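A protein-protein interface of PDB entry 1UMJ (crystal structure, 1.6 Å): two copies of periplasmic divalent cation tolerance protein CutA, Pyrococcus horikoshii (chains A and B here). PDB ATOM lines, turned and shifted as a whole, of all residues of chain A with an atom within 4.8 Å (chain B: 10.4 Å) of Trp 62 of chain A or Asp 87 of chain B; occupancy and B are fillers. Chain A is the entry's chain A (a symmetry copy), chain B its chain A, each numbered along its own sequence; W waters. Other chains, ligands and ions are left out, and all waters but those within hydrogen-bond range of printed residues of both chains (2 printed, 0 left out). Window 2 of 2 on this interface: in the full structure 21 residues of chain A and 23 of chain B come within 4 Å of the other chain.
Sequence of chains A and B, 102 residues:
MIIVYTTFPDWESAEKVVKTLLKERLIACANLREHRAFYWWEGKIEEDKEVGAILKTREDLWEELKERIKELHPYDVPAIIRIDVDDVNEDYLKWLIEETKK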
ATOM      1  N   ILE A   2      17.849   8.066  25.191  1.00  0.00           N
ATOM      2  CA  ILE A   2      16.567   8.684  25.580  1.00  0.00           C
ATOM      3  C   ILE A   2      16.531   8.758  27.099  1.00  0.00           C
ATOM      4  O   ILE A   2      17.332   8.072  27.786  1.00  0.00           O
ATOM      5  CB  ILE A   2      15.361   7.799  25.183  1.00  0.00           C
ATOM      6  CG1 ILE A   2      15.541   6.373  25.741  1.00  0.00           C
ATOM      7  CG2 ILE A   2      15.208   7.798  23.646  1.00  0.00           C
ATOM      8  CD1 ILE A   2      14.462   5.370  25.314  1.00  0.00           C
ATOM      9  N   VAL A   4      13.645   8.216  30.106  1.00  0.00           N
ATOM     10  CA  VAL A   4      12.311   7.660  30.279  1.00  0.00           C
ATOM     11  C   VAL A   4      11.922   7.991  31.673  1.00  0.00           C
ATOM     12  O   VAL A   4      12.700   7.780  32.600  1.00  0.00           O
ATOM     13  CB  VAL A   4      12.230   6.113  30.068  1.00  0.00           C
ATOM     14  CG1 VAL A   4      10.866   5.572  30.577  1.00  0.00           C
ATOM     15  CG2 VAL A   4      12.419   5.809  28.611  1.00  0.00           C
ATOM     16  N   ARG A  58      19.272   3.434  26.005  1.00  0.00           N
ATOM     17  CA  ARG A  58      19.396   3.571  24.554  1.00  0.00           C
ATOM     18  C   ARG A  58      18.035   3.751  23.847  1.00  0.00           C
ATOM     19  O   ARG A  58      16.983   3.240  24.260  1.00  0.00           O
ATOM     20  CB  ARG A  58      20.143   2.334  23.976  1.00  0.00           C
ATOM     21  CG  ARG A  58      21.540   2.057  24.465  1.00  0.00           C
ATOM     22  CD  ARG A  58      22.232   1.023  23.553  1.00  0.00           C
ATOM     23  NE  ARG A  58      21.358  -0.074  23.145  1.00  0.00           N
ATOM     24  CZ  ARG A  58      21.336  -1.269  23.721  1.00  0.00           C
ATOM     25  NH1 ARG A  58      22.143  -1.514  24.749  1.00  0.00           N
ATOM     26  NH2 ARG A  58      20.552  -2.241  23.245  1.00  0.00           N
ATOM     27  N   GLU A  59      18.068   4.482  22.746  1.00  0.00           N
ATOM     28  CA  GLU A  59      16.897   4.717  21.963  1.00  0.00           C
ATOM     29  C   GLU A  59      16.258   3.399  21.534  1.00  0.00           C
ATOM     30  O   GLU A  59      15.069   3.218  21.643  1.00  0.00           O
ATOM     31  CB  GLU A  59      17.261   5.570  20.736  1.00  0.00           C
ATOM     32  CG  GLU A  59      17.508   7.026  21.095  1.00  0.00           C
ATOM     33  CD  GLU A  59      18.049   7.871  19.962  1.00  0.00           C
ATOM     34  OE1 GLU A  59      17.708   7.633  18.766  1.00  0.00           O
ATOM     35  OE2 GLU A  59      18.810   8.796  20.281  1.00  0.00           O
ATOM     36  N   ASP A  60      17.083   2.442  21.138  1.00  0.00           N
ATOM     37  CA  ASP A  60      16.534   1.188  20.650  1.00  0.00           C
ATOM     38  C   ASP A  60      16.048   0.195  21.702  1.00  0.00           C
ATOM     39  O   ASP A  60      15.586  -0.881  21.359  1.00  0.00           O
ATOM     40  CB  ASP A  60      17.512   0.553  19.628  1.00  0.00           C
ATOM     41  CG  ASP A  60      18.730  -0.023  20.251  1.00  0.00           C
ATOM     42  OD1 ASP A  60      19.733  -0.263  19.519  1.00  0.00           O
ATOM     43  OD2 ASP A  60      18.700  -0.264  21.491  1.00  0.00           O
ATOM     44  N   LEU A  61      16.137   0.565  22.978  1.00  0.00           N
ATOM     45  CA  LEU A  61      15.659  -0.276  24.050  1.00  0.00           C
ATOM     46  C   LEU A  61      14.291   0.232  24.547  1.00  0.00           C
ATOM     47  O   LEU A  61      13.710  -0.362  25.467  1.00  0.00           O
ATOM     48  CB  LEU A  61      16.679  -0.327  25.200  1.00  0.00           C
ATOM     49  CG  LEU A  61      17.962  -1.131  24.945  1.00  0.00           C
ATOM     50  CD1 LEU A  61      18.861  -1.121  26.150  1.00  0.00           C
ATOM     51  CD2 LEU A  61      17.570  -2.581  24.601  1.00  0.00           C
ATOM     52  N   TRP A  62      13.765   1.301  23.927  1.00  0.00           N
ATOM     53  CA  TRP A  62      12.458   1.864  24.365  1.00  0.00           C
ATOM     54  C   TRP A  62      11.288   0.881  24.465  1.00  0.00           C
ATOM     55  O   TRP A  62      10.636   0.767  25.518  1.00  0.00           O
ATOM     56  CB  TRP A  62      12.049   3.036  23.467  1.00  0.00           C
ATOM     57  CG  TRP A  62      10.623   3.477  23.550  1.00  0.00           C
ATOM     58  CD1 TRP A  62       9.742   3.489  22.529  1.00  0.00           C
ATOM     59  CD2 TRP A  62       9.917   3.981  24.695  1.00  0.00           C
ATOM     60  NE1 TRP A  62       8.530   3.961  22.935  1.00  0.00           N
ATOM     61  CE2 TRP A  62       8.606   4.280  24.267  1.00  0.00           C
ATOM     62  CE3 TRP A  62      10.270   4.216  26.030  1.00  0.00           C
ATOM     63  CZ2 TRP A  62       7.641   4.800  25.117  1.00  0.00           C
ATOM     64  CZ3 TRP A  62       9.306   4.738  26.891  1.00  0.00           C
ATOM     65  CH2 TRP A  62       8.007   5.029  26.425  1.00  0.00           C
ATOM     66  N   GLU A  63      10.967   0.180  23.391  1.00  0.00           N
ATOM     67  CA  GLU A  63       9.830  -0.719  23.443  1.00  0.00           C
ATOM     68  C   GLU A  63       9.980  -1.857  24.467  1.00  0.00           C
ATOM     69  O   GLU A  63       9.018  -2.201  25.147  1.00  0.00           O
ATOM     70  CB  GLU A  63       9.572  -1.317  22.053  1.00  0.00           C
ATOM     71  CG  GLU A  63       9.130  -0.333  20.955  1.00  0.00           C
ATOM     72  CD  GLU A  63       7.797   0.322  21.221  1.00  0.00           C
ATOM     73  OE1 GLU A  63       7.065  -0.141  22.119  1.00  0.00           O
ATOM     74  OE2 GLU A  63       7.467   1.298  20.514  1.00  0.00           O
ATOM     75  N   GLU A  64      11.165  -2.451  24.574  1.00  0.00           N
ATOM     76  CA  GLU A  64      11.329  -3.523  25.542  1.00  0.00           C
ATOM     77  C   GLU A  64      11.204  -2.963  26.943  1.00  0.00           C
ATOM     78  O   GLU A  64      10.548  -3.561  27.811  1.00  0.00           O
ATOM     79  CB  GLU A  64      12.695  -4.199  25.408  1.00  0.00           C
ATOM     80  CG  GLU A  64      12.642  -5.644  25.909  1.00  0.00           C
ATOM     81  CD  GLU A  64      13.958  -6.362  25.803  1.00  0.00           C
ATOM     82  OE1 GLU A  64      14.747  -6.018  24.890  1.00  0.00           O
ATOM     83  OE2 GLU A  64      14.196  -7.287  26.618  1.00  0.00           O
ATOM     84  N   LEU A  65      11.818  -1.795  27.155  1.00  0.00           N
ATOM     85  CA  LEU A  65      11.782  -1.179  28.484  1.00  0.00           C
ATOM     86  C   LEU A  65      10.334  -0.834  28.863  1.00  0.00           C
ATOM     87  O   LEU A  65       9.891  -1.120  29.991  1.00  0.00           O
ATOM     88  CB  LEU A  65      12.693   0.055  28.497  1.00  0.00           C
ATOM     89  CG  LEU A  65      12.550   0.889  29.787  1.00  0.00           C
ATOM     90  CD1 LEU A  65      12.969   0.111  31.025  1.00  0.00           C
ATOM     91  CD2 LEU A  65      13.433   2.087  29.619  1.00  0.00           C
ATOM     92  N   LYS A  66       9.596  -0.208  27.947  1.00  0.00           N
ATOM     93  CA  LYS A  66       8.214   0.147  28.166  1.00  0.00           C
ATOM     94  C   LYS A  66       7.406  -1.108  28.555  1.00  0.00           C
ATOM     95  O   LYS A  66       6.648  -1.073  29.493  1.00  0.00           O
ATOM     96  CB  LYS A  66       7.617   0.771  26.889  1.00  0.00           C
ATOM     97  CG  LYS A  66       6.132   1.108  26.952  1.00  0.00           C
ATOM     98  CD  LYS A  66       5.582   1.706  25.655  1.00  0.00           C
ATOM     99  CE  LYS A  66       5.139   0.606  24.647  1.00  0.00           C
ATOM    100  NZ  LYS A  66       4.631   1.218  23.429  1.00  0.00           N
ATOM    101  N   ILE A  80       4.634   6.080  31.399  1.00  0.00           N
ATOM    102  CA  ILE A  80       5.936   5.654  30.891  1.00  0.00           C
ATOM    103  C   ILE A  80       6.168   6.651  29.746  1.00  0.00           C
ATOM    104  O   ILE A  80       5.654   6.501  28.632  1.00  0.00           O
ATOM    105  CB  ILE A  80       5.908   4.194  30.371  1.00  0.00           C
ATOM    106  CG1 ILE A  80       5.258   3.291  31.433  1.00  0.00           C
ATOM    107  CG2 ILE A  80       7.331   3.715  30.076  1.00  0.00           C
ATOM    108  CD1 ILE A  80       4.963   1.854  30.943  1.00  0.00           C
ATOM    109  N   ILE A  81       6.938   7.695  30.064  1.00  0.00           N
ATOM    110  CA  ILE A  81       7.163   8.796  29.146  1.00  0.00           C
ATOM    111  C   ILE A  81       8.569   8.846  28.547  1.00  0.00           C
ATOM    112  O   ILE A  81       9.583   8.762  29.263  1.00  0.00           O
ATOM    113  CB  ILE A  81       6.824  10.099  29.912  1.00  0.00           C
ATOM    114  CG1 ILE A  81       5.316  10.117  30.194  1.00  0.00           C
ATOM    115  CG2 ILE A  81       7.215  11.309  29.130  1.00  0.00           C
ATOM    116  CD1 ILE A  81       4.936  11.117  31.269  1.00  0.00           C
ATOM    117  N   ARG A  82       8.615   8.884  27.221  1.00  0.00           N
ATOM    118  CA  ARG A  82       9.893   8.908  26.501  1.00  0.00           C
ATOM    119  C   ARG A  82      10.261  10.323  26.022  1.00  0.00           C
ATOM    120  O   ARG A  82       9.476  10.932  25.312  1.00  0.00           O
ATOM    121  CB  ARG A  82       9.836   7.987  25.250  1.00  0.00           C
ATOM    122  CG  ARG A  82      11.096   8.129  24.384  1.00  0.00           C
ATOM    123  CD  ARG A  82      11.031   7.192  23.149  1.00  0.00           C
ATOM    124  NE  ARG A  82      11.963   7.637  22.148  1.00  0.00           N
ATOM    125  CZ  ARG A  82      12.346   6.863  21.142  1.00  0.00           C
ATOM    126  NH1 ARG A  82      11.844   5.631  21.051  1.00  0.00           N
ATOM    127  NH2 ARG A  82      13.231   7.305  20.263  1.00  0.00           N
ATOM    128  N   MET B   1       1.337  14.159  23.735  1.00  0.00           N
ATOM    129  CA  MET B   1       1.235  14.905  25.031  1.00  0.00           C
ATOM    130  C   MET B   1       2.482  15.740  25.197  1.00  0.00           C
ATOM    131  O   MET B   1       3.459  15.604  24.440  1.00  0.00           O
ATOM    132  CB  MET B   1       1.075  13.904  26.190  1.00  0.00           C
ATOM    133  CG  MET B   1       2.308  12.982  26.438  1.00  0.00           C
ATOM    134  SD  MET B   1       2.157  12.161  28.036  1.00  0.00           S
ATOM    135  CE  MET B   1       2.520  13.546  29.248  1.00  0.00           C
ATOM    136  N   ILE B   2       2.456  16.638  26.174  1.00  0.00           N
ATOM    137  CA  ILE B   2       3.661  17.455  26.415  1.00  0.00           C
ATOM    138  C   ILE B   2       3.887  17.512  27.918  1.00  0.00           C
ATOM    139  O   ILE B   2       2.965  17.191  28.711  1.00  0.00           O
ATOM    140  CB  ILE B   2       3.456  18.924  25.974  1.00  0.00           C
ATOM    141  CG1 ILE B   2       2.187  19.504  26.633  1.00  0.00           C
ATOM    142  CG2 ILE B   2       3.382  18.993  24.433  1.00  0.00           C
ATOM    143  CD1 ILE B   2       1.814  20.922  26.180  1.00  0.00           C
ATOM    144  N   ILE B   3       5.109  17.900  28.289  1.00  0.00           N
ATOM    145  CA  ILE B   3       5.446  18.215  29.677  1.00  0.00           C
ATOM    146  C   ILE B   3       5.627  19.742  29.667  1.00  0.00           C
ATOM    147  O   ILE B   3       6.122  20.338  28.694  1.00  0.00           O
ATOM    148  CB  ILE B   3       6.739  17.499  30.128  1.00  0.00           C
ATOM    149  CG1 ILE B   3       6.431  16.008  30.346  1.00  0.00           C
ATOM    150  CG2 ILE B   3       7.260  18.141  31.462  1.00  0.00           C
ATOM    151  CD1 ILE B   3       7.659  15.195  30.730  1.00  0.00           C
ATOM    152  N   GLU B  59      -0.982  18.139  23.984  1.00  0.00           N
ATOM    153  CA  GLU B  59      -0.275  19.002  23.093  1.00  0.00           C
ATOM    154  C   GLU B  59      -1.138  20.196  22.694  1.00  0.00           C
ATOM    155  O   GLU B  59      -0.696  21.320  22.714  1.00  0.00           O
ATOM    156  CB  GLU B  59       0.164  18.210  21.850  1.00  0.00           C
ATOM    157  CG  GLU B  59       1.334  17.283  22.137  1.00  0.00           C
ATOM    158  CD  GLU B  59       1.688  16.346  21.002  1.00  0.00           C
ATOM    159  OE1 GLU B  59       1.536  16.710  19.799  1.00  0.00           O
ATOM    160  OE2 GLU B  59       2.140  15.238  21.326  1.00  0.00           O
ATOM    161  N   ILE B  83       8.119  20.866  26.670  1.00  0.00           N
ATOM    162  CA  ILE B  83       8.959  19.771  26.168  1.00  0.00           C
ATOM    163  C   ILE B  83       7.989  18.735  25.574  1.00  0.00           C
ATOM    164  O   ILE B  83       7.109  18.194  26.255  1.00  0.00           O
ATOM    165  CB  ILE B  83       9.776  19.056  27.289  1.00  0.00           C
ATOM    166  CG1 ILE B  83      10.535  20.095  28.093  1.00  0.00           C
ATOM    167  CG2 ILE B  83      10.639  17.914  26.651  1.00  0.00           C
ATOM    168  CD1 ILE B  83      11.582  20.806  27.317  1.00  0.00           C
ATOM    169  N   ASP B  84       8.105  18.476  24.270  1.00  0.00           N
ATOM    170  CA  ASP B  84       7.251  17.466  23.643  1.00  0.00           C
ATOM    171  C   ASP B  84       7.673  16.053  24.063  1.00  0.00           C
ATOM    172  O   ASP B  84       8.859  15.778  24.248  1.00  0.00           O
ATOM    173  CB  ASP B  84       7.366  17.544  22.119  1.00  0.00           C
ATOM    174  CG  ASP B  84       6.960  18.862  21.571  1.00  0.00           C
ATOM    175  OD1 ASP B  84       6.093  19.508  22.190  1.00  0.00           O
ATOM    176  OD2 ASP B  84       7.503  19.233  20.497  1.00  0.00           O
ATOM    177  N   VAL B  85       6.698  15.186  24.285  1.00  0.00           N
ATOM    178  CA  VAL B  85       6.944  13.788  24.626  1.00  0.00           C
ATOM    179  C   VAL B  85       7.005  12.972  23.346  1.00  0.00           C
ATOM    180  O   VAL B  85       6.071  12.981  22.570  1.00  0.00           O
ATOM    181  CB  VAL B  85       5.860  13.266  25.624  1.00  0.00           C
ATOM    182  CG1 VAL B  85       6.005  11.771  25.859  1.00  0.00           C
ATOM    183  CG2 VAL B  85       6.045  13.998  26.964  1.00  0.00           C
ATOM    184  N   ASP B  86       8.100  12.267  23.117  1.00  0.00           N
ATOM    185  CA  ASP B  86       8.236  11.536  21.854  1.00  0.00           C
ATOM    186  C   ASP B  86       7.389  10.280  21.746  1.00  0.00           C
ATOM    187  O   ASP B  86       6.967   9.895  20.641  1.00  0.00           O
ATOM    188  CB  ASP B  86       9.697  11.261  21.632  1.00  0.00           C
ATOM    189  CG  ASP B  86      10.508  12.584  21.538  1.00  0.00           C
ATOM    190  OD1 ASP B  86      11.152  13.028  22.533  1.00  0.00           O
ATOM    191  OD2 ASP B  86      10.452  13.216  20.465  1.00  0.00           O
ATOM    192  N   ASP B  87       7.131   9.660  22.888  1.00  0.00           N
ATOM    193  CA  ASP B  87       6.267   8.494  22.914  1.00  0.00           C
ATOM    194  C   ASP B  87       5.853   8.237  24.344  1.00  0.00           C
ATOM    195  O   ASP B  87       6.480   8.710  25.297  1.00  0.00           O
ATOM    196  CB  ASP B  87       6.952   7.279  22.274  1.00  0.00           C
ATOM    197  CG  ASP B  87       5.941   6.171  21.866  1.00  0.00           C
ATOM    198  OD1 ASP B  87       4.712   6.398  21.890  1.00  0.00           O
ATOM    199  OD2 ASP B  87       6.402   5.059  21.533  1.00  0.00           O
ATOM    200  N   VAL B  88       4.758   7.516  24.489  1.00  0.00           N
ATOM    201  CA  VAL B  88       4.235   7.263  25.815  1.00  0.00           C
ATOM    202  C   VAL B  88       3.333   6.046  25.715  1.00  0.00           C
ATOM    203  O   VAL B  88       2.860   5.692  24.622  1.00  0.00           O
ATOM    204  CB  VAL B  88       3.470   8.507  26.317  1.00  0.00           C
ATOM    205  CG1 VAL B  88       2.368   8.871  25.294  1.00  0.00           C
ATOM    206  CG2 VAL B  88       2.850   8.248  27.683  1.00  0.00           C
ATOM    207  N   ASN B  89       3.135   5.356  26.823  1.00  0.00           N
ATOM    208  CA  ASN B  89       2.245   4.197  26.802  1.00  0.00           C
ATOM    209  C   ASN B  89       0.806   4.680  26.564  1.00  0.00           C
ATOM    210  O   ASN B  89       0.288   5.617  27.139  1.00  0.00           O
ATOM    211  CB  ASN B  89       2.396   3.334  28.090  1.00  0.00           C
ATOM    212  CG  ASN B  89       2.127   4.115  29.366  1.00  0.00           C
ATOM    213  OD1 ASN B  89       2.669   5.178  29.544  1.00  0.00           O
ATOM    214  ND2 ASN B  89       1.282   3.597  30.244  1.00  0.00           N
ATOM    215  N   GLU B  90       0.148   4.003  25.640  1.00  0.00           N
ATOM    216  CA  GLU B  90      -1.177   4.366  25.244  1.00  0.00           C
ATOM    217  C   GLU B  90      -2.254   4.482  26.317  1.00  0.00           C
ATOM    218  O   GLU B  90      -3.071   5.412  26.292  1.00  0.00           O
ATOM    219  CB  GLU B  90      -1.579   3.401  24.113  1.00  0.00           C
ATOM    220  CG  GLU B  90      -2.884   3.720  23.441  1.00  0.00           C
ATOM    221  CD  GLU B  90      -2.858   5.029  22.660  1.00  0.00           C
ATOM    222  OE1 GLU B  90      -3.959   5.570  22.443  1.00  0.00           O
ATOM    223  OE2 GLU B  90      -1.767   5.508  22.285  1.00  0.00           O
ATOM    224  N   ASP B  91      -2.264   3.568  27.290  1.00  0.00           N
ATOM    225  CA  ASP B  91      -3.283   3.647  28.310  1.00  0.00           C
ATOM    226  C   ASP B  91      -3.129   4.889  29.152  1.00  0.00           C
ATOM    227  O   ASP B  91      -4.110   5.481  29.611  1.00  0.00           O
ATOM    228  CB  ASP B  91      -3.249   2.401  29.163  1.00  0.00           C
ATOM    229  CG  ASP B  91      -3.885   1.233  28.461  1.00  0.00           C
ATOM    230  OD1 ASP B  91      -3.812   0.107  28.982  1.00  0.00           O
ATOM    231  OD2 ASP B  91      -4.449   1.472  27.380  1.00  0.00           O
ATOM    232  N   TYR B  92      -1.876   5.318  29.338  1.00  0.00           N
ATOM    233  CA  TYR B  92      -1.655   6.527  30.110  1.00  0.00           C
ATOM    234  C   TYR B  92      -2.093   7.742  29.291  1.00  0.00           C
ATOM    235  O   TYR B  92      -2.726   8.661  29.825  1.00  0.00           O
ATOM    236  CB  TYR B  92      -0.168   6.656  30.518  1.00  0.00           C
ATOM    237  CG  TYR B  92       0.081   7.951  31.255  1.00  0.00           C
ATOM    238  CD1 TYR B  92      -0.203   8.052  32.608  1.00  0.00           C
ATOM    239  CD2 TYR B  92       0.519   9.102  30.564  1.00  0.00           C
ATOM    240  CE1 TYR B  92      -0.074   9.263  33.264  1.00  0.00           C
ATOM    241  CE2 TYR B  92       0.652  10.312  31.214  1.00  0.00           C
ATOM    242  CZ  TYR B  92       0.352  10.386  32.569  1.00  0.00           C
ATOM    243  OH  TYR B  92       0.501  11.595  33.212  1.00  0.00           O
ATOM    244  N   LEU B  93      -1.783   7.747  27.984  1.00  0.00           N
ATOM    245  CA  LEU B  93      -2.210   8.849  27.140  1.00  0.00           C
ATOM    246  C   LEU B  93      -3.749   8.957  27.169  1.00  0.00           C
ATOM    247  O   LEU B  93      -4.301  10.051  27.266  1.00  0.00           O
ATOM    248  CB  LEU B  93      -1.733   8.624  25.705  1.00  0.00           C
ATOM    249  CG  LEU B  93      -2.219   9.685  24.728  1.00  0.00           C
ATOM    250  CD1 LEU B  93      -1.860  11.087  25.226  1.00  0.00           C
ATOM    251  CD2 LEU B  93      -1.611   9.437  23.381  1.00  0.00           C
ATOM    252  N   LEU B  96      -4.821  10.620  30.370  1.00  0.00           N
ATOM    253  CA  LEU B  96      -4.531  12.049  30.319  1.00  0.00           C
ATOM    254  C   LEU B  96      -5.523  12.900  29.472  1.00  0.00           C
ATOM    255  O   LEU B  96      -5.911  14.028  29.860  1.00  0.00           O
ATOM    256  CB  LEU B  96      -3.060  12.220  29.851  1.00  0.00           C
ATOM    257  CG  LEU B  96      -2.554  13.665  29.658  1.00  0.00           C
ATOM    258  CD1 LEU B  96      -1.030  13.668  29.838  1.00  0.00           C
ATOM    259  CD2 LEU B  96      -2.979  14.283  28.298  1.00  0.00           C
HETATM  260  O   HOH W   1       3.924   3.489  22.806  1.00  0.00           O
HETATM  261  O   HOH W   2       1.777   1.368  24.612  1.00  0.00           O
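Printed residues of chain B within 4 Å of Trp 62 of chain A: Asp 87. Of chain A, only Trp 62 (2.8 Å), Ile 81 (3.9 Å) and Arg 82 (2.9 Å) come within 4 Å of Asp 87 of chain B. Leu 61 of chain A touches none of the printed residues of chain B. No residue of chain B comes within 4 Å of Glu 63 of chain A. No residue of chain B comes within 4 Å of Leu 65 of chain A. No residue of chain B comes within 4 Å of Lys 66 of chain A. Of the printed residues of chain A, Val 88 of chain B touches Ile 80 (3.2 Å) and Ile 81 (3.98 Å). Of the printed residues of chain A, Met 1 of chain B touches Ile 81 (3.98 Å). Glu 90 of chain B touches none of the printed residues of chain A. Leu 93 of chain B touches none of the printed residues of chain A. The nearest printed residue of chain B that does not touch Trp 62 of chain A is Val 88 of chain B (4.01 Å). The nearest printed residue of chain A that does not touch Val 88 of chain B is Trp 62 of chain A (4.01 Å).
The backbone carbonyl oxygen (O) of Arg 82 of chain A lies within hydrogen-bond range of the backbone NH (N) of Asp 86 of chain B. The side-chain carboxylate of Asp 87 of chain B sits at hydrogen-bond distance from the indole nitrogen of Trp 62 of chain A. The backbone carbonyl oxygen (O) of Asp 87 of chain B sits at hydrogen-bond distance from the backbone NH (N) of Arg 82 of chain A (2.9 Å). OD1 of Asn 89 of chain B sits at hydrogen-bond distance from N of Ile 80 of chain A.
Water W1 lies within hydrogen-bond range of the side-chain amino group (NZ) of Lys 66 of chain A, the backbone carbonyl oxygen (O) of Val 88 of chain B and the side-chain carboxylate (OD1) of Asp 87 of chain B. Water W2 bridges the side-chain amino group (NZ) of Lys 66 of chain A (3.1 Å) and the backbone NH (N) of Glu 90 of chain B (3.3 Å).
2 positions are printed for both chains. Of the 10 pairs that touch across the chains among the printed residues, none has its exchanged pair printed and touching as well.
Among the printed residues, pairs that only touch across the chains: Ile 80 of chain A with Val 88 of chain B, Ile 81 of chain A with Val 85 of chain B, Arg 82 of chain A with Val 85 of chain B, Ile 81 of chain A with Asp 87 of chain B, Ile 81 of chain A with Met 1 of chain B and Ile 81 of chain A with Val 88 of chain B.
Hydrophobic or aromatic side chains of chain A within 4 Å of the printed part of chain B: Trp 62, Ile 80 and Ile 81. Printed residues of chain B that touch a printed residue of chain A: Met 1, Val 85, Asp 86, Asp 87, Val 88 and Asn 89. Hydrophobic or aromatic side chains of chain B that line the printed part of chain A: Met 1, Val 85 and Val 88. Along chain B the printed residues that touch a printed residue of chain A span positions 1 to 89. Among the printed residues, no Asp or Glu carboxylate lies within 4 Å of a Lys or Arg side-chain nitrogen of the other chain.
N of Met 1 of chain B sits at hydrogen-bond distance from OE2 of Glu 59 of chain B, at 2.8 Å. N of Val 85 of chain B is in hydrogen-bond range of O of Met 1 of chain B (3.3 Å).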
